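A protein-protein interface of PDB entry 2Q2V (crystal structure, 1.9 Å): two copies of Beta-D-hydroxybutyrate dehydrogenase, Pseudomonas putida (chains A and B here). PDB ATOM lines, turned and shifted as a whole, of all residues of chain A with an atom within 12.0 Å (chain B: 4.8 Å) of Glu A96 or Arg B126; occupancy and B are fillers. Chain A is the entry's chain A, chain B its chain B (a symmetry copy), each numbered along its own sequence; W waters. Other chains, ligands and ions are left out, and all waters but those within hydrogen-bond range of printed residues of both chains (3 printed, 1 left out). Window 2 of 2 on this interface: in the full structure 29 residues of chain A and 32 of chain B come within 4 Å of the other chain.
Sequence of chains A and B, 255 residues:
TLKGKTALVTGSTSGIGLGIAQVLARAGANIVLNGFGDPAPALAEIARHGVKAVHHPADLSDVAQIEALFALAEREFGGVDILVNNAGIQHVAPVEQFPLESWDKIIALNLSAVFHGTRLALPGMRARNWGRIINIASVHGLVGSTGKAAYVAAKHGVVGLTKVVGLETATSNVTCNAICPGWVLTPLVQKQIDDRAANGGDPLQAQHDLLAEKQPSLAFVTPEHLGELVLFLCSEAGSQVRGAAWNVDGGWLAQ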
ATOM      1  N   HIS A  91      30.171  -3.897 -10.659  1.00  0.00           N
ATOM      2  CA  HIS A  91      29.011  -3.050 -10.777  1.00  0.00           C
ATOM      3  C   HIS A  91      28.534  -3.073 -12.218  1.00  0.00           C
ATOM      4  O   HIS A  91      29.326  -2.916 -13.129  1.00  0.00           O
ATOM      5  CB  HIS A  91      29.306  -1.613 -10.328  1.00  0.00           C
ATOM      6  CG  HIS A  91      28.093  -0.732 -10.320  1.00  0.00           C
ATOM      7  ND1 HIS A  91      27.655  -0.033 -11.431  1.00  0.00           N
ATOM      8  CD2 HIS A  91      27.193  -0.487  -9.343  1.00  0.00           C
ATOM      9  CE1 HIS A  91      26.562   0.637 -11.114  1.00  0.00           C
ATOM     10  NE2 HIS A  91      26.265   0.388  -9.855  1.00  0.00           N
ATOM     11  N   VAL A  92      27.229  -3.238 -12.410  1.00  0.00           N
ATOM     12  CA  VAL A  92      26.698  -3.372 -13.762  1.00  0.00           C
ATOM     13  C   VAL A  92      25.853  -2.163 -14.163  1.00  0.00           C
ATOM     14  O   VAL A  92      24.896  -1.791 -13.461  1.00  0.00           O
ATOM     15  CB  VAL A  92      25.885  -4.686 -13.900  1.00  0.00           C
ATOM     16  CG1 VAL A  92      25.161  -4.723 -15.249  1.00  0.00           C
ATOM     17  CG2 VAL A  92      26.838  -5.905 -13.716  1.00  0.00           C
ATOM     18  N   ALA A  93      26.224  -1.526 -15.281  1.00  0.00           N
ATOM     19  CA  ALA A  93      25.448  -0.408 -15.812  1.00  0.00           C
ATOM     20  C   ALA A  93      25.961  -0.114 -17.203  1.00  0.00           C
ATOM     21  O   ALA A  93      27.127  -0.379 -17.471  1.00  0.00           O
ATOM     22  CB  ALA A  93      25.601   0.826 -14.921  1.00  0.00           C
ATOM     23  N   PRO A  94      25.099   0.423 -18.087  1.00  0.00           N
ATOM     24  CA  PRO A  94      25.617   0.856 -19.392  1.00  0.00           C
ATOM     25  C   PRO A  94      26.713   1.922 -19.218  1.00  0.00           C
ATOM     26  O   PRO A  94      26.669   2.754 -18.271  1.00  0.00           O
ATOM     27  CB  PRO A  94      24.391   1.484 -20.085  1.00  0.00           C
ATOM     28  CG  PRO A  94      23.206   1.081 -19.335  1.00  0.00           C
ATOM     29  CD  PRO A  94      23.648   0.666 -17.944  1.00  0.00           C
ATOM     30  N   VAL A  95      27.655   1.933 -20.149  1.00  0.00           N
ATOM     31  CA  VAL A  95      28.811   2.796 -20.034  1.00  0.00           C
ATOM     32  C   VAL A  95      28.386   4.259 -19.781  1.00  0.00           C
ATOM     33  O   VAL A  95      28.954   4.911 -18.886  1.00  0.00           O
ATOM     34  CB  VAL A  95      29.810   2.592 -21.237  1.00  0.00           C
ATOM     35  CG1 VAL A  95      29.210   3.190 -22.538  1.00  0.00           C
ATOM     36  CG2 VAL A  95      31.225   3.206 -20.896  1.00  0.00           C
ATOM     37  N   GLU A  96      27.352   4.748 -20.489  1.00  0.00           N
ATOM     38  CA  GLU A  96      27.001   6.155 -20.367  1.00  0.00           C
ATOM     39  C   GLU A  96      26.305   6.508 -19.052  1.00  0.00           C
ATOM     40  O   GLU A  96      26.094   7.675 -18.765  1.00  0.00           O
ATOM     41  CB  GLU A  96      26.260   6.716 -21.606  1.00  0.00           C
ATOM     42  CG  GLU A  96      24.842   6.195 -21.869  1.00  0.00           C
ATOM     43  CD  GLU A  96      24.846   4.910 -22.677  1.00  0.00           C
ATOM     44  OE1 GLU A  96      24.068   4.844 -23.651  1.00  0.00           O
ATOM     45  OE2 GLU A  96      25.636   3.977 -22.359  1.00  0.00           O
ATOM     46  N   GLN A  97      25.921   5.487 -18.288  1.00  0.00           N
ATOM     47  CA  GLN A  97      25.259   5.697 -17.005  1.00  0.00           C
ATOM     48  C   GLN A  97      26.110   5.061 -15.901  1.00  0.00           C
ATOM     49  O   GLN A  97      25.654   4.911 -14.760  1.00  0.00           O
ATOM     50  CB  GLN A  97      23.874   5.042 -17.025  1.00  0.00           C
ATOM     51  CG  GLN A  97      23.012   5.449 -18.200  1.00  0.00           C
ATOM     52  CD  GLN A  97      21.796   4.540 -18.395  1.00  0.00           C
ATOM     53  OE1 GLN A  97      21.411   3.745 -17.499  1.00  0.00           O
ATOM     54  NE2 GLN A  97      21.174   4.658 -19.566  1.00  0.00           N
ATOM     55  N   PHE A  98      27.343   4.678 -16.252  1.00  0.00           N
ATOM     56  CA  PHE A  98      28.209   4.000 -15.278  1.00  0.00           C
ATOM     57  C   PHE A  98      28.645   5.048 -14.243  1.00  0.00           C
ATOM     58  O   PHE A  98      29.240   6.056 -14.595  1.00  0.00           O
ATOM     59  CB  PHE A  98      29.407   3.320 -15.922  1.00  0.00           C
ATOM     60  CG  PHE A  98      29.924   2.119 -15.144  1.00  0.00           C
ATOM     61  CD1 PHE A  98      29.577   0.806 -15.526  1.00  0.00           C
ATOM     62  CD2 PHE A  98      30.766   2.301 -14.044  1.00  0.00           C
ATOM     63  CE1 PHE A  98      30.056  -0.322 -14.811  1.00  0.00           C
ATOM     64  CE2 PHE A  98      31.266   1.194 -13.335  1.00  0.00           C
ATOM     65  CZ  PHE A  98      30.889  -0.126 -13.713  1.00  0.00           C
ATOM     66  N   PRO A  99      28.338   4.809 -12.961  1.00  0.00           N
ATOM     67  CA  PRO A  99      28.652   5.817 -11.934  1.00  0.00           C
ATOM     68  C   PRO A  99      30.154   6.083 -11.803  1.00  0.00           C
ATOM     69  O   PRO A  99      30.968   5.157 -11.835  1.00  0.00           O
ATOM     70  CB  PRO A  99      28.119   5.178 -10.641  1.00  0.00           C
ATOM     71  CG  PRO A  99      27.034   4.213 -11.117  1.00  0.00           C
ATOM     72  CD  PRO A  99      27.643   3.639 -12.390  1.00  0.00           C
ATOM     73  N   LEU A 100      30.498   7.352 -11.641  1.00  0.00           N
ATOM     74  CA  LEU A 100      31.892   7.740 -11.573  1.00  0.00           C
ATOM     75  C   LEU A 100      32.552   7.122 -10.354  1.00  0.00           C
ATOM     76  O   LEU A 100      33.659   6.629 -10.426  1.00  0.00           O
ATOM     77  CB  LEU A 100      31.981   9.265 -11.511  1.00  0.00           C
ATOM     78  CG  LEU A 100      31.791  10.092 -12.804  1.00  0.00           C
ATOM     79  CD1 LEU A 100      30.593   9.682 -13.679  1.00  0.00           C
ATOM     80  CD2 LEU A 100      31.687  11.528 -12.413  1.00  0.00           C
ATOM     81  N   GLU A 101      31.863   7.092  -9.220  1.00  0.00           N
ATOM     82  CA  GLU A 101      32.509   6.531  -8.039  1.00  0.00           C
ATOM     83  C   GLU A 101      32.723   5.029  -8.184  1.00  0.00           C
ATOM     84  O   GLU A 101      33.637   4.459  -7.613  1.00  0.00           O
ATOM     85  CB  GLU A 101      31.727   6.911  -6.779  1.00  0.00           C
ATOM     86  CG  GLU A 101      30.481   6.139  -6.565  1.00  0.00           C
ATOM     87  CD  GLU A 101      29.681   6.725  -5.431  1.00  0.00           C
ATOM     88  OE1 GLU A 101      30.061   6.520  -4.254  1.00  0.00           O
ATOM     89  OE2 GLU A 101      28.693   7.404  -5.733  1.00  0.00           O
ATOM     90  N   SER A 102      31.861   4.377  -8.949  1.00  0.00           N
ATOM     91  CA  SER A 102      31.979   2.942  -9.094  1.00  0.00           C
ATOM     92  C   SER A 102      33.108   2.597 -10.082  1.00  0.00           C
ATOM     93  O   SER A 102      33.864   1.634  -9.894  1.00  0.00           O
ATOM     94  CB  SER A 102      30.583   2.385  -9.425  1.00  0.00           C
ATOM     95  OG  SER A 102      30.744   1.246 -10.197  1.00  0.00           O
ATOM     96  N   TRP A 103      33.275   3.421 -11.108  1.00  0.00           N
ATOM     97  CA  TRP A 103      34.412   3.265 -12.027  1.00  0.00           C
ATOM     98  C   TRP A 103      35.704   3.365 -11.190  1.00  0.00           C
ATOM     99  O   TRP A 103      36.592   2.520 -11.302  1.00  0.00           O
ATOM    100  CB  TRP A 103      34.353   4.364 -13.147  1.00  0.00           C
ATOM    101  CG  TRP A 103      35.641   4.399 -13.950  1.00  0.00           C
ATOM    102  CD1 TRP A 103      36.775   5.109 -13.653  1.00  0.00           C
ATOM    103  CD2 TRP A 103      35.938   3.631 -15.128  1.00  0.00           C
ATOM    104  NE1 TRP A 103      37.744   4.870 -14.609  1.00  0.00           N
ATOM    105  CE2 TRP A 103      37.268   3.954 -15.515  1.00  0.00           C
ATOM    106  CE3 TRP A 103      35.194   2.750 -15.927  1.00  0.00           C
ATOM    107  CZ2 TRP A 103      37.888   3.368 -16.641  1.00  0.00           C
ATOM    108  CZ3 TRP A 103      35.800   2.172 -17.052  1.00  0.00           C
ATOM    109  CH2 TRP A 103      37.140   2.488 -17.400  1.00  0.00           C
ATOM    110  N   SER A 145      31.791  -7.955 -21.759  1.00  0.00           N
ATOM    111  CA  SER A 145      30.355  -8.228 -21.637  1.00  0.00           C
ATOM    112  C   SER A 145      29.708  -6.870 -21.538  1.00  0.00           C
ATOM    113  O   SER A 145      30.335  -5.917 -21.052  1.00  0.00           O
ATOM    114  CB  SER A 145      30.022  -9.030 -20.385  1.00  0.00           C
ATOM    115  OG  SER A 145      30.468 -10.372 -20.550  1.00  0.00           O
ATOM    116  N   THR A 146      28.453  -6.786 -21.952  1.00  0.00           N
ATOM    117  CA  THR A 146      27.661  -5.592 -21.717  1.00  0.00           C
ATOM    118  C   THR A 146      27.523  -5.286 -20.212  1.00  0.00           C
ATOM    119  O   THR A 146      27.386  -6.197 -19.367  1.00  0.00           O
ATOM    120  CB  THR A 146      26.271  -5.696 -22.341  1.00  0.00           C
ATOM    121  OG1 THR A 146      25.634  -6.895 -21.906  1.00  0.00           O
ATOM    122  CG2 THR A 146      26.360  -5.686 -23.901  1.00  0.00           C
ATOM    123  N   GLY A 147      27.531  -3.996 -19.901  1.00  0.00           N
ATOM    124  CA  GLY A 147      27.251  -3.498 -18.559  1.00  0.00           C
ATOM    125  C   GLY A 147      28.425  -3.537 -17.623  1.00  0.00           C
ATOM    126  O   GLY A 147      28.319  -3.074 -16.474  1.00  0.00           O
ATOM    127  N   LYS A 148      29.567  -4.054 -18.094  1.00  0.00           N
ATOM    128  CA  LYS A 148      30.712  -4.239 -17.211  1.00  0.00           C
ATOM    129  C   LYS A 148      31.933  -3.362 -17.582  1.00  0.00           C
ATOM    130  O   LYS A 148      33.065  -3.813 -17.434  1.00  0.00           O
ATOM    131  CB  LYS A 148      31.105  -5.745 -17.124  1.00  0.00           C
ATOM    132  CG  LYS A 148      30.031  -6.596 -16.381  1.00  0.00           C
ATOM    133  CD  LYS A 148      30.425  -8.114 -16.258  1.00  0.00           C
ATOM    134  CE  LYS A 148      29.169  -8.858 -15.680  1.00  0.00           C
ATOM    135  NZ  LYS A 148      29.425 -10.271 -15.269  1.00  0.00           N
ATOM    136  N   ALA A 149      31.711  -2.108 -18.022  1.00  0.00           N
ATOM    137  CA  ALA A 149      32.834  -1.254 -18.478  1.00  0.00           C
ATOM    138  C   ALA A 149      34.073  -1.251 -17.533  1.00  0.00           C
ATOM    139  O   ALA A 149      35.240  -1.452 -17.969  1.00  0.00           O
ATOM    140  CB  ALA A 149      32.353   0.187 -18.749  1.00  0.00           C
ATOM    141  N   ALA A 150      33.830  -0.938 -16.263  1.00  0.00           N
ATOM    142  CA  ALA A 150      34.966  -0.739 -15.347  1.00  0.00           C
ATOM    143  C   ALA A 150      35.668  -2.046 -15.031  1.00  0.00           C
ATOM    144  O   ALA A 150      36.900  -2.101 -14.924  1.00  0.00           O
ATOM    145  CB  ALA A 150      34.514  -0.036 -14.054  1.00  0.00           C
ATOM    146  N   ARG B 119      31.585   8.268 -22.118  1.00  0.00           N
ATOM    147  CA  ARG B 119      30.330   8.456 -21.405  1.00  0.00           C
ATOM    148  C   ARG B 119      29.654   9.806 -21.773  1.00  0.00           C
ATOM    149  O   ARG B 119      28.415   9.920 -21.843  1.00  0.00           O
ATOM    150  CB  ARG B 119      30.470   8.224 -19.874  1.00  0.00           C
ATOM    151  CG  ARG B 119      30.966   9.415 -19.112  1.00  0.00           C
ATOM    152  CD  ARG B 119      31.040   9.192 -17.582  1.00  0.00           C
ATOM    153  NE  ARG B 119      31.767  10.344 -17.065  1.00  0.00           N
ATOM    154  CZ  ARG B 119      31.248  11.537 -16.782  1.00  0.00           C
ATOM    155  NH1 ARG B 119      29.939  11.782 -16.910  1.00  0.00           N
ATOM    156  NH2 ARG B 119      32.059  12.492 -16.332  1.00  0.00           N
ATOM    157  N   LEU B 122      28.515   9.457 -25.831  1.00  0.00           N
ATOM    158  CA  LEU B 122      27.622   8.411 -26.361  1.00  0.00           C
ATOM    159  C   LEU B 122      26.128   8.826 -26.396  1.00  0.00           C
ATOM    160  O   LEU B 122      25.459   8.493 -27.362  1.00  0.00           O
ATOM    161  CB  LEU B 122      27.780   7.087 -25.596  1.00  0.00           C
ATOM    162  CG  LEU B 122      27.048   5.850 -26.096  1.00  0.00           C
ATOM    163  CD1 LEU B 122      27.328   5.666 -27.611  1.00  0.00           C
ATOM    164  CD2 LEU B 122      27.582   4.624 -25.334  1.00  0.00           C
ATOM    165  N   PRO B 123      25.614   9.507 -25.354  1.00  0.00           N
ATOM    166  CA  PRO B 123      24.190   9.838 -25.401  1.00  0.00           C
ATOM    167  C   PRO B 123      23.780  10.617 -26.649  1.00  0.00           C
ATOM    168  O   PRO B 123      22.747  10.307 -27.214  1.00  0.00           O
ATOM    169  CB  PRO B 123      23.988  10.716 -24.165  1.00  0.00           C
ATOM    170  CG  PRO B 123      25.053  10.248 -23.207  1.00  0.00           C
ATOM    171  CD  PRO B 123      26.229   9.969 -24.081  1.00  0.00           C
ATOM    172  N   GLY B 124      24.550  11.625 -27.050  1.00  0.00           N
ATOM    173  CA  GLY B 124      24.220  12.425 -28.245  1.00  0.00           C
ATOM    174  C   GLY B 124      24.378  11.650 -29.563  1.00  0.00           C
ATOM    175  O   GLY B 124      23.606  11.845 -30.497  1.00  0.00           O
ATOM    176  N   MET B 125      25.380  10.783 -29.637  1.00  0.00           N
ATOM    177  CA  MET B 125      25.550   9.842 -30.761  1.00  0.00           C
ATOM    178  C   MET B 125      24.335   8.926 -30.918  1.00  0.00           C
ATOM    179  O   MET B 125      23.771   8.799 -32.009  1.00  0.00           O
ATOM    180  CB  MET B 125      26.807   9.001 -30.538  1.00  0.00           C
ATOM    181  CG  MET B 125      28.060   9.814 -30.801  1.00  0.00           C
ATOM    182  SD  MET B 125      29.532   8.854 -30.410  1.00  0.00           S
ATOM    183  CE  MET B 125      30.804  10.083 -30.767  1.00  0.00           C
ATOM    184  N   ARG B 126      23.921   8.303 -29.824  1.00  0.00           N
ATOM    185  CA  ARG B 126      22.686   7.522 -29.810  1.00  0.00           C
ATOM    186  C   ARG B 126      21.470   8.339 -30.253  1.00  0.00           C
ATOM    187  O   ARG B 126      20.666   7.884 -31.107  1.00  0.00           O
ATOM    188  CB  ARG B 126      22.456   6.919 -28.410  1.00  0.00           C
ATOM    189  CG  ARG B 126      23.350   5.696 -28.128  1.00  0.00           C
ATOM    190  CD  ARG B 126      22.800   4.986 -26.900  1.00  0.00           C
ATOM    191  NE  ARG B 126      23.636   3.915 -26.337  1.00  0.00           N
ATOM    192  CZ  ARG B 126      23.660   2.655 -26.786  1.00  0.00           C
ATOM    193  NH1 ARG B 126      22.944   2.291 -27.865  1.00  0.00           N
ATOM    194  NH2 ARG B 126      24.417   1.754 -26.172  1.00  0.00           N
ATOM    195  N   ALA B 127      21.338   9.529 -29.665  1.00  0.00           N
ATOM    196  CA  ALA B 127      20.182  10.371 -29.879  1.00  0.00           C
ATOM    197  C   ALA B 127      20.105  10.840 -31.319  1.00  0.00           C
ATOM    198  O   ALA B 127      19.019  11.041 -31.822  1.00  0.00           O
ATOM    199  CB  ALA B 127      20.197  11.573 -28.920  1.00  0.00           C
ATOM    200  N   ARG B 128      21.252  11.020 -31.975  1.00  0.00           N
ATOM    201  CA  ARG B 128      21.268  11.452 -33.367  1.00  0.00           C
ATOM    202  C   ARG B 128      21.472  10.305 -34.341  1.00  0.00           C
ATOM    203  O   ARG B 128      21.664  10.537 -35.541  1.00  0.00           O
ATOM    204  CB  ARG B 128      22.299  12.557 -33.621  1.00  0.00           C
ATOM    205  CG  ARG B 128      21.951  13.856 -32.933  1.00  0.00           C
ATOM    206  CD  ARG B 128      23.160  14.784 -32.978  1.00  0.00           C
ATOM    207  NE  ARG B 128      24.249  14.151 -32.234  1.00  0.00           N
ATOM    208  CZ  ARG B 128      25.524  14.487 -32.284  1.00  0.00           C
ATOM    209  NH1 ARG B 128      25.953  15.487 -33.085  1.00  0.00           N
ATOM    210  NH2 ARG B 128      26.375  13.799 -31.526  1.00  0.00           N
ATOM    211  N   ASN B 129      21.419   9.077 -33.836  1.00  0.00           N
ATOM    212  CA  ASN B 129      21.370   7.893 -34.723  1.00  0.00           C
ATOM    213  C   ASN B 129      22.643   7.631 -35.524  1.00  0.00           C
ATOM    214  O   ASN B 129      22.601   7.009 -36.590  1.00  0.00           O
ATOM    215  CB  ASN B 129      20.155   8.015 -35.689  1.00  0.00           C
ATOM    216  CG  ASN B 129      19.816   6.673 -36.390  1.00  0.00           C
ATOM    217  OD1 ASN B 129      19.946   5.609 -35.780  1.00  0.00           O
ATOM    218  ND2 ASN B 129      19.418   6.733 -37.670  1.00  0.00           N
ATOM    219  N   GLU B 168      27.768  -2.919 -26.369  1.00  0.00           N
ATOM    220  CA  GLU B 168      26.648  -2.155 -25.874  1.00  0.00           C
ATOM    221  C   GLU B 168      25.964  -1.356 -26.986  1.00  0.00           C
ATOM    222  O   GLU B 168      24.738  -1.141 -26.959  1.00  0.00           O
ATOM    223  CB  GLU B 168      27.083  -1.234 -24.729  1.00  0.00           C
ATOM    224  CG  GLU B 168      27.317  -2.005 -23.424  1.00  0.00           C
ATOM    225  CD  GLU B 168      27.541  -1.090 -22.221  1.00  0.00           C
ATOM    226  OE1 GLU B 168      27.396   0.153 -22.391  1.00  0.00           O
ATOM    227  OE2 GLU B 168      27.849  -1.623 -21.121  1.00  0.00           O
ATOM    228  N   THR B 169      26.776  -0.908 -27.941  1.00  0.00           N
ATOM    229  CA  THR B 169      26.260  -0.128 -29.062  1.00  0.00           C
ATOM    230  C   THR B 169      25.984  -0.935 -30.314  1.00  0.00           C
ATOM    231  O   THR B 169      25.694  -0.352 -31.366  1.00  0.00           O
ATOM    232  CB  THR B 169      27.218   1.049 -29.437  1.00  0.00           C
ATOM    233  OG1 THR B 169      28.546   0.560 -29.720  1.00  0.00           O
ATOM    234  CG2 THR B 169      27.254   2.055 -28.305  1.00  0.00           C
ATOM    235  N   SER B 172      23.003  -0.336 -32.662  1.00  0.00           N
ATOM    236  CA  SER B 172      22.829   1.050 -33.073  1.00  0.00           C
ATOM    237  C   SER B 172      23.738   1.377 -34.246  1.00  0.00           C
ATOM    238  O   SER B 172      24.556   0.554 -34.634  1.00  0.00           O
ATOM    239  CB  SER B 172      23.197   1.958 -31.906  1.00  0.00           C
ATOM    240  OG  SER B 172      24.611   2.012 -31.738  1.00  0.00           O
ATOM    241  N   VAL B 174      26.076   3.438 -33.835  1.00  0.00           N
ATOM    242  CA  VAL B 174      27.286   3.922 -33.205  1.00  0.00           C
ATOM    243  C   VAL B 174      28.249   2.754 -33.117  1.00  0.00           C
ATOM    244  O   VAL B 174      27.851   1.661 -32.702  1.00  0.00           O
ATOM    245  CB  VAL B 174      27.004   4.499 -31.770  1.00  0.00           C
ATOM    246  CG1 VAL B 174      28.302   5.037 -31.108  1.00  0.00           C
ATOM    247  CG2 VAL B 174      25.859   5.573 -31.850  1.00  0.00           C
HETATM  248  O   HOH W   1      27.557   9.754 -17.146  1.00  0.00           O
HETATM  249  O   HOH W   2      26.681  10.759 -19.930  1.00  0.00           O
HETATM  250  O   HOH W   3      25.611   1.563 -23.638  1.00  0.00           O
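Hydrophobic or aromatic side chains of chain A that line the printed part of chain B: Val A95 and Leu A100.
Hydrophobic or aromatic side chains of chain B that line the printed part of chain A: Leu B122.
Among the printed residues, 11 pairs touch across the chains.
Water W3 lies within hydrogen-bond range of the side-chain carboxylate (OE1) of Glu B168 (2.6 Å), the side-chain carboxylate (OE2) of Glu A96 (2.7 Å) and the guanidinium group (NH2) of Arg B126 (2.8 Å).
Water W2 bridges the backbone carbonyl oxygen of Arg B119 (2.7 Å) and the backbone carbonyl oxygen of Glu A96 (3.3 Å).
Water W1 lies within hydrogen-bond range of the backbone carbonyl oxygen of Glu A96 (3.0 Å) and the guanidinium group of Arg B119 (3.1 Å).
Among the printed residues, merely in contact across the chains: Val A95 with Leu B122 (3.5 Å), Pro A94 with Glu B168 (3.6 Å), Glu A96 with Leu B122 (3.6 Å), Leu A100 with Arg B119 (3.6 Å), Val A95 with Arg B119 (3.8 Å), Thr A146 with Glu B168 (3.8 Å), Glu A96 with Arg B119 (3.9 Å) and Ala A93 with Glu B168 (3.9 Å).
No position is printed for both chains.
Of the 11 pairs that touch across the chains among the printed residues, none has its exchanged pair printed and touching as well.
Of the printed residues of chain B, Ala A93 touches Glu B168 (3.9 Å).
Glu A96 touches three residues of chain B.
Of the printed residues of chain B, Leu A100 touches Arg B119.
Printed residues of chain B within 4 Å of Thr A146: Glu B168 (3.8 Å).
Of the printed residues of chain B, Gly A147 touches Glu B168.
Of the printed residues of chain A, Arg B119 touches Val A95, Glu A96 and Leu A100.
Of chain A, only Val A95 and Glu A96 come within 4 Å of Leu B122.
No residue of chain A comes within 4 Å of Pro B123.
Arg B126 touches just one residue of chain A: Glu A96 (2.9 Å).
No residue of chain A comes within 4 Å of Ala B127.
No residue of chain A comes within 4 Å of Asn B129.
No residue of chain A comes within 4 Å of Thr B169.
No residue of chain A comes within 4 Å of Ser B172.
No residue of chain A comes within 4 Å of Val B174.
The nearest residue of chain B that does not touch Glu A96 is Pro B123 (4.1 Å).
The nearest residue of chain A that does not touch Arg B126 is Pro A94 (6.1 Å).
O of Gly A147 lies within hydrogen-bond range of N of Ala A93, 2.9 Å away.
The guanidinium group (NH2) of Arg B126 lies within hydrogen-bond range of the backbone carbonyl oxygen (O) of Glu B168 (3.0 Å).
The side-chain carboxylate of Glu A96 is in salt-bridge range of the guanidinium group of Arg B126 (2.9 Å).
N of Gly A147 lies within hydrogen-bond range of OE2 of Glu B168, 2.7 Å away.
N of Val A95 sits at hydrogen-bond distance from OE1 of Glu B168 (2.9 Å).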
